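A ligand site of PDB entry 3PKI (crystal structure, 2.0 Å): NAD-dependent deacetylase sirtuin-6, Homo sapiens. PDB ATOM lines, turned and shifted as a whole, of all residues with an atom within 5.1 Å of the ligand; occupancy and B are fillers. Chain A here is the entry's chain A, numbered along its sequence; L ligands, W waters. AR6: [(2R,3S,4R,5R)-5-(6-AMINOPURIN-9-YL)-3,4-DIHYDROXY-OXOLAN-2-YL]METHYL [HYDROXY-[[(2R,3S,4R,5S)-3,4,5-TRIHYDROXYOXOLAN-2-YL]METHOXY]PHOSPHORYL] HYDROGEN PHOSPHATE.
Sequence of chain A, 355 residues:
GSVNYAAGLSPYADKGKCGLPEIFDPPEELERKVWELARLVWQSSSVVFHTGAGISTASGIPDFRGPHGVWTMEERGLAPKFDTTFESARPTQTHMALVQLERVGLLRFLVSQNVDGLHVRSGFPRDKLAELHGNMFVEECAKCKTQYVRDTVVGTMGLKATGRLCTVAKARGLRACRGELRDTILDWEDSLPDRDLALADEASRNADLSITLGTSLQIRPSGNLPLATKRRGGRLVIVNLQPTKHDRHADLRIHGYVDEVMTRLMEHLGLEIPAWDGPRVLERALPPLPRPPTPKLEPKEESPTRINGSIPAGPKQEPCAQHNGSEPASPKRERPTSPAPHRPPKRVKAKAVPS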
ATOM      1  N   GLU A  22      21.194  -0.150  25.657  1.00  0.00           N
ATOM      2  CA  GLU A  22      20.600  -1.152  26.553  1.00  0.00           C
ATOM      3  C   GLU A  22      19.141  -0.821  26.861  1.00  0.00           C
ATOM      4  O   GLU A  22      18.758   0.350  26.872  1.00  0.00           O
ATOM      5  CB  GLU A  22      21.395  -1.246  27.851  1.00  0.00           C
ATOM      6  CG  GLU A  22      22.749  -1.903  27.688  1.00  0.00           C
ATOM      7  CD  GLU A  22      23.515  -2.073  28.978  1.00  0.00           C
ATOM      8  OE1 GLU A  22      23.548  -1.116  29.795  1.00  0.00           O
ATOM      9  OE2 GLU A  22      24.104  -3.159  29.171  1.00  0.00           O
ATOM     10  N   GLY A  52      25.485 -16.886  26.223  1.00  0.00           N
ATOM     11  CA  GLY A  52      26.451 -16.067  25.517  1.00  0.00           C
ATOM     12  C   GLY A  52      27.292 -15.271  26.498  1.00  0.00           C
ATOM     13  O   GLY A  52      27.140 -15.397  27.714  1.00  0.00           O
ATOM     14  N   ALA A  53      28.175 -14.439  25.954  1.00  0.00           N
ATOM     15  CA  ALA A  53      29.166 -13.633  26.658  1.00  0.00           C
ATOM     16  C   ALA A  53      28.605 -12.712  27.778  1.00  0.00           C
ATOM     17  O   ALA A  53      29.350 -12.338  28.679  1.00  0.00           O
ATOM     18  CB  ALA A  53      29.961 -12.813  25.657  1.00  0.00           C
ATOM     19  N   GLY A  54      27.308 -12.388  27.726  1.00  0.00           N
ATOM     20  CA  GLY A  54      26.664 -11.540  28.725  1.00  0.00           C
ATOM     21  C   GLY A  54      26.618 -12.120  30.139  1.00  0.00           C
ATOM     22  O   GLY A  54      26.569 -11.357  31.108  1.00  0.00           O
ATOM     23  N   THR A  57      30.146 -11.150  32.072  1.00  0.00           N
ATOM     24  CA  THR A  57      30.541  -9.732  32.278  1.00  0.00           C
ATOM     25  C   THR A  57      30.600  -9.392  33.770  1.00  0.00           C
ATOM     26  O   THR A  57      31.497  -8.666  34.175  1.00  0.00           O
ATOM     27  CB  THR A  57      29.657  -8.769  31.495  1.00  0.00           C
ATOM     28  OG1 THR A  57      28.307  -8.916  31.936  1.00  0.00           O
ATOM     29  CG2 THR A  57      29.753  -8.954  29.980  1.00  0.00           C
ATOM     30  N   ASP A  63      31.943  -8.594  27.125  1.00  0.00           N
ATOM     31  CA  ASP A  63      31.222  -9.321  26.091  1.00  0.00           C
ATOM     32  C   ASP A  63      31.782  -8.861  24.725  1.00  0.00           C
ATOM     33  O   ASP A  63      32.848  -8.240  24.679  1.00  0.00           O
ATOM     34  CB  ASP A  63      29.685  -9.163  26.216  1.00  0.00           C
ATOM     35  CG  ASP A  63      29.164  -7.742  26.123  1.00  0.00           C
ATOM     36  OD1 ASP A  63      28.043  -7.504  26.573  1.00  0.00           O
ATOM     37  OD2 ASP A  63      29.895  -6.865  25.605  1.00  0.00           O
ATOM     38  N   PHE A  64      31.077  -9.129  23.627  1.00  0.00           N
ATOM     39  CA  PHE A  64      31.578  -8.742  22.328  1.00  0.00           C
ATOM     40  C   PHE A  64      30.891  -7.519  21.745  1.00  0.00           C
ATOM     41  O   PHE A  64      31.569  -6.684  21.144  1.00  0.00           O
ATOM     42  CB  PHE A  64      31.461  -9.924  21.335  1.00  0.00           C
ATOM     43  CG  PHE A  64      32.450 -11.013  21.633  1.00  0.00           C
ATOM     44  CD1 PHE A  64      32.093 -12.105  22.420  1.00  0.00           C
ATOM     45  CD2 PHE A  64      33.762 -10.937  21.161  1.00  0.00           C
ATOM     46  CE1 PHE A  64      33.022 -13.101  22.732  1.00  0.00           C
ATOM     47  CE2 PHE A  64      34.693 -11.939  21.466  1.00  0.00           C
ATOM     48  CZ  PHE A  64      34.322 -13.015  22.244  1.00  0.00           C
ATOM     49  N   ARG A  65      29.551  -7.427  21.884  1.00  0.00           N
ATOM     50  CA  ARG A  65      28.745  -6.389  21.250  1.00  0.00           C
ATOM     51  C   ARG A  65      27.990  -5.435  22.215  1.00  0.00           C
ATOM     52  O   ARG A  65      27.219  -4.600  21.745  1.00  0.00           O
ATOM     53  CB  ARG A  65      27.766  -7.035  20.253  1.00  0.00           C
ATOM     54  CG  ARG A  65      28.503  -7.815  19.162  1.00  0.00           C
ATOM     55  CD  ARG A  65      27.596  -8.628  18.260  1.00  0.00           C
ATOM     56  NE  ARG A  65      28.365  -9.471  17.351  1.00  0.00           N
ATOM     57  CZ  ARG A  65      28.800 -10.702  17.631  1.00  0.00           C
ATOM     58  NH1 ARG A  65      28.555 -11.247  18.825  1.00  0.00           N
ATOM     59  NH2 ARG A  65      29.492 -11.390  16.726  1.00  0.00           N
ATOM     60  N   GLY A  66      28.276  -5.510  23.511  1.00  0.00           N
ATOM     61  CA  GLY A  66      27.662  -4.611  24.484  1.00  0.00           C
ATOM     62  C   GLY A  66      28.256  -3.207  24.398  1.00  0.00           C
ATOM     63  O   GLY A  66      29.202  -3.003  23.630  1.00  0.00           O
ATOM     64  N   TRP A  71      34.219  -6.225  20.282  1.00  0.00           N
ATOM     65  CA  TRP A  71      34.039  -5.710  18.918  1.00  0.00           C
ATOM     66  C   TRP A  71      33.655  -4.227  18.951  1.00  0.00           C
ATOM     67  O   TRP A  71      34.246  -3.440  18.200  1.00  0.00           O
ATOM     68  CB  TRP A  71      33.031  -6.526  18.098  1.00  0.00           C
ATOM     69  CG  TRP A  71      33.274  -8.009  17.994  1.00  0.00           C
ATOM     70  CD1 TRP A  71      32.319  -8.976  17.858  1.00  0.00           C
ATOM     71  CD2 TRP A  71      34.545  -8.700  17.936  1.00  0.00           C
ATOM     72  NE1 TRP A  71      32.901 -10.219  17.748  1.00  0.00           N
ATOM     73  CE2 TRP A  71      34.269 -10.079  17.799  1.00  0.00           C
ATOM     74  CE3 TRP A  71      35.891  -8.285  18.023  1.00  0.00           C
ATOM     75  CZ2 TRP A  71      35.285 -11.044  17.756  1.00  0.00           C
ATOM     76  CZ3 TRP A  71      36.894  -9.245  17.986  1.00  0.00           C
ATOM     77  CH2 TRP A  71      36.591 -10.603  17.845  1.00  0.00           C
ATOM     78  N   GLN A 113      28.068 -20.376  23.628  1.00  0.00           N
ATOM     79  CA  GLN A 113      28.902 -19.751  22.606  1.00  0.00           C
ATOM     80  C   GLN A 113      30.170 -19.198  23.280  1.00  0.00           C
ATOM     81  O   GLN A 113      31.041 -18.665  22.590  1.00  0.00           O
ATOM     82  CB  GLN A 113      28.131 -18.609  21.938  1.00  0.00           C
ATOM     83  CG  GLN A 113      26.958 -19.076  21.096  1.00  0.00           C
ATOM     84  CD  GLN A 113      26.095 -17.912  20.667  1.00  0.00           C
ATOM     85  OE1 GLN A 113      26.420 -17.190  19.727  1.00  0.00           O
ATOM     86  NE2 GLN A 113      24.996 -17.692  21.383  1.00  0.00           N
ATOM     87  N   ASN A 114      30.255 -19.315  24.613  1.00  0.00           N
ATOM     88  CA  ASN A 114      31.383 -18.819  25.407  1.00  0.00           C
ATOM     89  C   ASN A 114      32.590 -19.708  25.319  1.00  0.00           C
ATOM     90  O   ASN A 114      32.477 -20.932  25.401  1.00  0.00           O
ATOM     91  CB  ASN A 114      30.979 -18.639  26.863  1.00  0.00           C
ATOM     92  CG  ASN A 114      29.946 -17.585  27.030  1.00  0.00           C
ATOM     93  OD1 ASN A 114      29.661 -16.828  26.106  1.00  0.00           O
ATOM     94  ND2 ASN A 114      29.321 -17.520  28.202  1.00  0.00           N
ATOM     95  N   HIS A 133      31.748 -22.699  20.156  1.00  0.00           N
ATOM     96  CA  HIS A 133      32.837 -21.864  19.647  1.00  0.00           C
ATOM     97  C   HIS A 133      34.191 -22.204  20.246  1.00  0.00           C
ATOM     98  O   HIS A 133      35.201 -21.553  19.924  1.00  0.00           O
ATOM     99  CB  HIS A 133      32.499 -20.369  19.820  1.00  0.00           C
ATOM    100  CG  HIS A 133      31.220 -19.944  19.149  1.00  0.00           C
ATOM    101  ND1 HIS A 133      30.662 -18.717  19.390  1.00  0.00           N
ATOM    102  CD2 HIS A 133      30.436 -20.609  18.250  1.00  0.00           C
ATOM    103  CE1 HIS A 133      29.564 -18.663  18.651  1.00  0.00           C
ATOM    104  NE2 HIS A 133      29.389 -19.781  17.958  1.00  0.00           N
ATOM    105  N   TRP A 188      37.076 -17.203  12.400  1.00  0.00           N
ATOM    106  CA  TRP A 188      35.928 -16.844  11.552  1.00  0.00           C
ATOM    107  C   TRP A 188      35.636 -17.848  10.410  1.00  0.00           C
ATOM    108  O   TRP A 188      34.469 -18.144  10.169  1.00  0.00           O
ATOM    109  CB  TRP A 188      36.085 -15.431  10.980  1.00  0.00           C
ATOM    110  CG  TRP A 188      36.062 -14.361  12.031  1.00  0.00           C
ATOM    111  CD1 TRP A 188      37.124 -13.649  12.503  1.00  0.00           C
ATOM    112  CD2 TRP A 188      34.910 -13.897  12.759  1.00  0.00           C
ATOM    113  NE1 TRP A 188      36.701 -12.753  13.467  1.00  0.00           N
ATOM    114  CE2 TRP A 188      35.348 -12.877  13.645  1.00  0.00           C
ATOM    115  CE3 TRP A 188      33.546 -14.240  12.755  1.00  0.00           C
ATOM    116  CZ2 TRP A 188      34.477 -12.206  14.511  1.00  0.00           C
ATOM    117  CZ3 TRP A 188      32.676 -13.570  13.606  1.00  0.00           C
ATOM    118  CH2 TRP A 188      33.141 -12.564  14.474  1.00  0.00           C
ATOM    119  N   GLY A 214      22.119 -13.662  28.089  1.00  0.00           N
ATOM    120  CA  GLY A 214      23.253 -12.845  27.706  1.00  0.00           C
ATOM    121  C   GLY A 214      23.861 -13.108  26.344  1.00  0.00           C
ATOM    122  O   GLY A 214      25.092 -13.114  26.206  1.00  0.00           O
ATOM    123  N   THR A 215      23.014 -13.317  25.338  1.00  0.00           N
ATOM    124  CA  THR A 215      23.461 -13.489  23.950  1.00  0.00           C
ATOM    125  C   THR A 215      22.618 -12.586  23.038  1.00  0.00           C
ATOM    126  O   THR A 215      21.389 -12.544  23.154  1.00  0.00           O
ATOM    127  CB  THR A 215      23.527 -14.967  23.501  1.00  0.00           C
ATOM    128  OG1 THR A 215      23.835 -15.018  22.097  1.00  0.00           O
ATOM    129  CG2 THR A 215      22.247 -15.758  23.797  1.00  0.00           C
ATOM    130  N   SER A 216      23.292 -11.848  22.133  1.00  0.00           N
ATOM    131  CA  SER A 216      22.612 -10.981  21.159  1.00  0.00           C
ATOM    132  C   SER A 216      22.011 -11.820  19.990  1.00  0.00           C
ATOM    133  O   SER A 216      21.281 -11.285  19.160  1.00  0.00           O
ATOM    134  CB  SER A 216      23.558  -9.909  20.631  1.00  0.00           C
ATOM    135  OG  SER A 216      24.679 -10.503  19.981  1.00  0.00           O
ATOM    136  N   LEU A 217      22.350 -13.146  19.943  1.00  0.00           N
ATOM    137  CA  LEU A 217      21.866 -14.156  18.952  1.00  0.00           C
ATOM    138  C   LEU A 217      22.177 -13.774  17.477  1.00  0.00           C
ATOM    139  O   LEU A 217      21.460 -14.206  16.573  1.00  0.00           O
ATOM    140  CB  LEU A 217      20.350 -14.438  19.138  1.00  0.00           C
ATOM    141  CG  LEU A 217      19.903 -14.991  20.496  1.00  0.00           C
ATOM    142  CD1 LEU A 217      18.401 -14.827  20.674  1.00  0.00           C
ATOM    143  CD2 LEU A 217      20.314 -16.456  20.664  1.00  0.00           C
ATOM    144  N   GLN A 218      23.271 -13.019  17.262  1.00  0.00           N
ATOM    145  CA  GLN A 218      23.694 -12.501  15.944  1.00  0.00           C
ATOM    146  C   GLN A 218      24.560 -13.488  15.133  1.00  0.00           C
ATOM    147  O   GLN A 218      24.696 -13.307  13.914  1.00  0.00           O
ATOM    148  CB  GLN A 218      24.445 -11.179  16.124  1.00  0.00           C
ATOM    149  CG  GLN A 218      23.553 -10.025  16.574  1.00  0.00           C
ATOM    150  CD  GLN A 218      24.251  -8.694  16.514  1.00  0.00           C
ATOM    151  OE1 GLN A 218      24.700  -8.243  15.456  1.00  0.00           O
ATOM    152  NE2 GLN A 218      24.334  -8.002  17.640  1.00  0.00           N
ATOM    153  N   ILE A 219      25.148 -14.508  15.781  1.00  0.00           N
ATOM    154  CA  ILE A 219      26.008 -15.483  15.104  1.00  0.00           C
ATOM    155  C   ILE A 219      25.202 -16.679  14.667  1.00  0.00           C
ATOM    156  O   ILE A 219      24.431 -17.229  15.459  1.00  0.00           O
ATOM    157  CB  ILE A 219      27.237 -15.852  16.010  1.00  0.00           C
ATOM    158  CG1 ILE A 219      28.220 -14.657  16.131  1.00  0.00           C
ATOM    159  CG2 ILE A 219      27.970 -17.141  15.561  1.00  0.00           C
ATOM    160  CD1 ILE A 219      28.985 -14.187  14.778  1.00  0.00           C
ATOM    161  N   VAL A 239      16.575 -13.449  27.643  1.00  0.00           N
ATOM    162  CA  VAL A 239      17.020 -12.594  28.746  1.00  0.00           C
ATOM    163  C   VAL A 239      18.269 -11.881  28.248  1.00  0.00           C
ATOM    164  O   VAL A 239      19.278 -12.534  27.972  1.00  0.00           O
ATOM    165  CB  VAL A 239      17.302 -13.369  30.076  1.00  0.00           C
ATOM    166  CG1 VAL A 239      17.791 -12.412  31.167  1.00  0.00           C
ATOM    167  CG2 VAL A 239      16.086 -14.147  30.535  1.00  0.00           C
ATOM    168  N   ASN A 240      18.198 -10.550  28.117  1.00  0.00           N
ATOM    169  CA  ASN A 240      19.303  -9.757  27.568  1.00  0.00           C
ATOM    170  C   ASN A 240      19.088  -8.280  27.825  1.00  0.00           C
ATOM    171  O   ASN A 240      17.952  -7.811  27.822  1.00  0.00           O
ATOM    172  CB  ASN A 240      19.402  -9.985  26.054  1.00  0.00           C
ATOM    173  CG  ASN A 240      20.793  -9.844  25.532  1.00  0.00           C
ATOM    174  OD1 ASN A 240      21.726 -10.538  25.952  1.00  0.00           O
ATOM    175  ND2 ASN A 240      20.984  -8.925  24.617  1.00  0.00           N
ATOM    176  N   LEU A 241      20.187  -7.527  28.015  1.00  0.00           N
ATOM    177  CA  LEU A 241      20.113  -6.085  28.215  1.00  0.00           C
ATOM    178  C   LEU A 241      19.906  -5.317  26.894  1.00  0.00           C
ATOM    179  O   LEU A 241      19.225  -4.301  26.884  1.00  0.00           O
ATOM    180  CB  LEU A 241      21.354  -5.566  28.958  1.00  0.00           C
ATOM    181  CG  LEU A 241      21.338  -5.792  30.481  1.00  0.00           C
ATOM    182  CD1 LEU A 241      22.689  -5.454  31.082  1.00  0.00           C
ATOM    183  CD2 LEU A 241      20.219  -4.997  31.149  1.00  0.00           C
ATOM    184  N   GLN A 242      20.477  -5.822  25.795  1.00  0.00           N
ATOM    185  CA  GLN A 242      20.326  -5.177  24.488  1.00  0.00           C
ATOM    186  C   GLN A 242      19.239  -5.882  23.701  1.00  0.00           C
ATOM    187  O   GLN A 242      18.914  -7.039  24.031  1.00  0.00           O
ATOM    188  CB  GLN A 242      21.645  -5.300  23.686  1.00  0.00           C
ATOM    189  CG  GLN A 242      22.706  -4.262  24.031  1.00  0.00           C
ATOM    190  CD  GLN A 242      23.978  -4.515  23.255  1.00  0.00           C
ATOM    191  OE1 GLN A 242      24.319  -5.643  22.884  1.00  0.00           O
ATOM    192  NE2 GLN A 242      24.706  -3.459  22.968  1.00  0.00           N
ATOM    193  N   PRO A 243      18.723  -5.269  22.578  1.00  0.00           N
ATOM    194  CA  PRO A 243      17.807  -6.030  21.725  1.00  0.00           C
ATOM    195  C   PRO A 243      18.588  -7.168  21.064  1.00  0.00           C
ATOM    196  O   PRO A 243      19.806  -7.047  20.880  1.00  0.00           O
ATOM    197  CB  PRO A 243      17.331  -5.011  20.662  1.00  0.00           C
ATOM    198  CG  PRO A 243      17.931  -3.702  21.033  1.00  0.00           C
ATOM    199  CD  PRO A 243      19.019  -3.940  22.015  1.00  0.00           C
ATOM    200  N   GLY A 256      16.994  -7.208  31.779  1.00  0.00           N
ATOM    201  CA  GLY A 256      17.613  -7.000  33.082  1.00  0.00           C
ATOM    202  C   GLY A 256      18.940  -7.725  33.202  1.00  0.00           C
ATOM    203  O   GLY A 256      19.295  -8.519  32.314  1.00  0.00           O
ATOM    204  N   TYR A 257      19.678  -7.462  34.303  1.00  0.00           N
ATOM    205  CA  TYR A 257      20.957  -8.149  34.588  1.00  0.00           C
ATOM    206  C   TYR A 257      20.643  -9.601  34.853  1.00  0.00           C
ATOM    207  O   TYR A 257      19.763  -9.902  35.671  1.00  0.00           O
ATOM    208  CB  TYR A 257      21.709  -7.495  35.740  1.00  0.00           C
ATOM    209  CG  TYR A 257      22.143  -6.076  35.424  1.00  0.00           C
ATOM    210  CD1 TYR A 257      23.322  -5.830  34.721  1.00  0.00           C
ATOM    211  CD2 TYR A 257      21.363  -4.989  35.794  1.00  0.00           C
ATOM    212  CE1 TYR A 257      23.717  -4.526  34.403  1.00  0.00           C
ATOM    213  CE2 TYR A 257      21.749  -3.688  35.475  1.00  0.00           C
ATOM    214  CZ  TYR A 257      22.923  -3.465  34.779  1.00  0.00           C
ATOM    215  OH  TYR A 257      23.291  -2.176  34.466  1.00  0.00           O
ATOM    216  N   VAL A 258      21.277 -10.498  34.095  1.00  0.00           N
ATOM    217  CA  VAL A 258      21.029 -11.940  34.181  1.00  0.00           C
ATOM    218  C   VAL A 258      21.219 -12.478  35.632  1.00  0.00           C
ATOM    219  O   VAL A 258      20.405 -13.301  36.076  1.00  0.00           O
ATOM    220  CB  VAL A 258      21.796 -12.748  33.087  1.00  0.00           C
ATOM    221  CG1 VAL A 258      23.319 -12.718  33.284  1.00  0.00           C
ATOM    222  CG2 VAL A 258      21.264 -14.158  32.966  1.00  0.00           C
HETATM  223  N1  AR6 L   1      22.844  -9.354  31.894  1.00  0.00           N
HETATM  224  C2  AR6 L   1      22.120  -9.474  30.756  1.00  0.00           C
HETATM  225  N3  AR6 L   1      22.609  -9.212  29.536  1.00  0.00           N
HETATM  226  C4  AR6 L   1      23.911  -8.821  29.391  1.00  0.00           C
HETATM  227  C5  AR6 L   1      24.777  -8.694  30.564  1.00  0.00           C
HETATM  228  C6  AR6 L   1      24.144  -8.964  31.884  1.00  0.00           C
HETATM  229  N6  AR6 L   1      24.876  -8.870  33.023  1.00  0.00           N
HETATM  230  N7  AR6 L   1      25.986  -8.285  30.125  1.00  0.00           N
HETATM  231  C8  AR6 L   1      25.909  -8.189  28.772  1.00  0.00           C
HETATM  232  N9  AR6 L   1      24.659  -8.496  28.345  1.00  0.00           N
HETATM  233  PA  AR6 L   1      27.430 -10.564  22.409  1.00  0.00           P
HETATM  234  PB  AR6 L   1      27.446 -13.406  22.150  1.00  0.00           P
HETATM  235  C1' AR6 L   1      24.189  -8.657  26.964  1.00  0.00           C
HETATM  236  O1A AR6 L   1      28.354  -9.552  23.067  1.00  0.00           O
HETATM  237  O1B AR6 L   1      26.017 -13.287  21.704  1.00  0.00           O
HETATM  238  C1D AR6 L   1      31.499 -13.500  18.874  1.00  0.00           C
HETATM  239  O1D AR6 L   1      32.116 -13.328  17.590  1.00  0.00           O
HETATM  240  C2' AR6 L   1      24.690  -7.604  26.007  1.00  0.00           C
HETATM  241  O2' AR6 L   1      23.688  -6.594  25.979  1.00  0.00           O
HETATM  242  O2A AR6 L   1      27.122 -10.467  20.947  1.00  0.00           O
HETATM  243  O2B AR6 L   1      27.817 -14.528  23.083  1.00  0.00           O
HETATM  244  C2D AR6 L   1      32.067 -14.698  19.636  1.00  0.00           C
HETATM  245  O2D AR6 L   1      32.404 -15.729  18.687  1.00  0.00           O
HETATM  246  C3' AR6 L   1      24.830  -8.350  24.684  1.00  0.00           C
HETATM  247  O3' AR6 L   1      23.694  -8.135  23.840  1.00  0.00           O
HETATM  248  O3A AR6 L   1      28.003 -12.032  22.764  1.00  0.00           O
HETATM  249  C3D AR6 L   1      30.850 -15.158  20.424  1.00  0.00           C
HETATM  250  O3D AR6 L   1      30.948 -16.526  20.829  1.00  0.00           O
HETATM  251  C4' AR6 L   1      24.819  -9.833  25.059  1.00  0.00           C
HETATM  252  O4' AR6 L   1      24.674  -9.910  26.481  1.00  0.00           O
HETATM  253  C4D AR6 L   1      29.723 -14.956  19.417  1.00  0.00           C
HETATM  254  O4D AR6 L   1      30.111 -13.777  18.688  1.00  0.00           O
HETATM  255  C5' AR6 L   1      26.091 -10.519  24.639  1.00  0.00           C
HETATM  256  O5' AR6 L   1      26.057 -10.613  23.216  1.00  0.00           O
HETATM  257  C5D AR6 L   1      28.363 -14.756  20.078  1.00  0.00           C
HETATM  258  O5D AR6 L   1      28.377 -13.542  20.846  1.00  0.00           O
HETATM  259  O   HOH W   1      24.973  -4.784  27.363  1.00  0.00           O
HETATM  260  O   HOH W   2      27.551  -5.294  27.976  1.00  0.00           O
HETATM  261  O   HOH W   3      24.526 -10.358  35.517  1.00  0.00           O
HETATM  262  O   HOH W   4      27.176 -11.330  33.771  1.00  0.00           O
HETATM  263  O   HOH W   5      30.173 -15.844  23.495  1.00  0.00           O
HETATM  264  O   HOH W   6      34.698 -16.753  19.714  1.00  0.00           O
HETATM  265  O   HOH W   7      25.496 -12.917  19.099  1.00  0.00           O
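A ring nitrogen (ND1) of His 133 is in hydrogen-bond range of the backbone carbonyl oxygen (O) of Gln 113 (3.2 Å).
ND2 of Asn 240 sits at hydrogen-bond distance from O of Gln 242.
The side-chain hydroxyl (OG1) of Thr 215 lies close to the backbone NH (N) of Leu 217 (3.2 Å).
N of Ala 53 lies within hydrogen-bond range of O of Gly 214 (3.4 Å).
The backbone NH (N) of Ala 53 is in hydrogen-bond range of the side-chain amide oxygen (OD1) of Asn 114.
O of Gly 54 sits at hydrogen-bond distance from OG1 of Thr 57, at 3.1 Å.
The side-chain carboxylate of Asp 63 sits at hydrogen-bond distance from the backbone NH of Gly 66, 3.0 Å away.
ND2 of Asn 114 sits at hydrogen-bond distance from O of Gly 52 (3.1 Å).
Water W1 lies within hydrogen-bond range of the side-chain carboxylate (OE2) of Glu 22 (2.6 Å) and an oxygen (O2') of the ligand (2.6 Å).
Water W5 lies within hydrogen-bond range of O2B of the ligand, OD1 of Asn 114, O of Gln 113 and N of Ala 53.
Water W4 lies within hydrogen-bond range of O of Gly 54, OG1 of Thr 57 and N6 of the ligand.
The backbone NH of Ser 216 lies within hydrogen-bond range of an oxygen (O1B) of the ligand, 3.1 Å away.
An oxygen (O2A) of the ligand sits at hydrogen-bond distance from the side-chain hydroxyl (OG) of Ser 216, at 2.6 Å.
An oxygen (O3D) of the ligand sits at hydrogen-bond distance from a ring nitrogen (ND1) of His 133, at 2.6 Å.
An oxygen (O1A) of the ligand sits at hydrogen-bond distance from the backbone NH (N) of Arg 65 (2.7 Å).
O2A of the ligand is in salt-bridge range of NH1 of Arg 65.
N of Gln 242 lies close to O2' of the ligand.
OE1 of Gln 242 lies within hydrogen-bond range of O3' of the ligand (2.7 Å).
O of Gln 113 lies within hydrogen-bond range of O3D of the ligand.
The backbone NH of Phe 64 is in hydrogen-bond range of an oxygen (O1A) of the ligand, 2.8 Å away.
The side-chain hydroxyl (OG1) of Thr 215 lies within hydrogen-bond range of an oxygen (O1B) of the ligand, at 2.8 Å.
N of Ala 53 lies within hydrogen-bond range of O2B of the ligand (2.9 Å).
An oxygen (O3') of the ligand sits at hydrogen-bond distance from the side-chain amide nitrogen of Asn 240 (2.9 Å).
A nitrogen (N1) of the ligand lies within hydrogen-bond range of the backbone NH (N) of Val 258 (2.9 Å).
The side-chain hydroxyl (OG1) of Thr 57 lies within hydrogen-bond range of a nitrogen (N7) of the ligand (3.0 Å).
O1D of the ligand sits at hydrogen-bond distance from NE1 of Trp 71 (3.2 Å).
The backbone NH of Leu 241 sits at hydrogen-bond distance from a nitrogen (N3) of the ligand.
The backbone carbonyl oxygen (O) of Gly 54 sits close to a nitrogen (N7) of the ligand, at 3.3 Å.
O of Gly 214 lies close to O4' of the ligand, at 3.2 Å.
Gly 52 touches the ligand (CA to O2B, 3.2 Å).
Asp 63 touches the ligand.
Trp 188 touches the ligand.
CG1 of Ile 219 touches O4D of the ligand, 3.3 Å away.
Gly 256 touches the ligand.
Tyr 257 touches the ligand.
Hydrophobic or aromatic side chains that line the ligand: Ala 53, Phe 64, Trp 71, His 133, Trp 188, Ile 219, Leu 241, Tyr 257 and Val 258.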
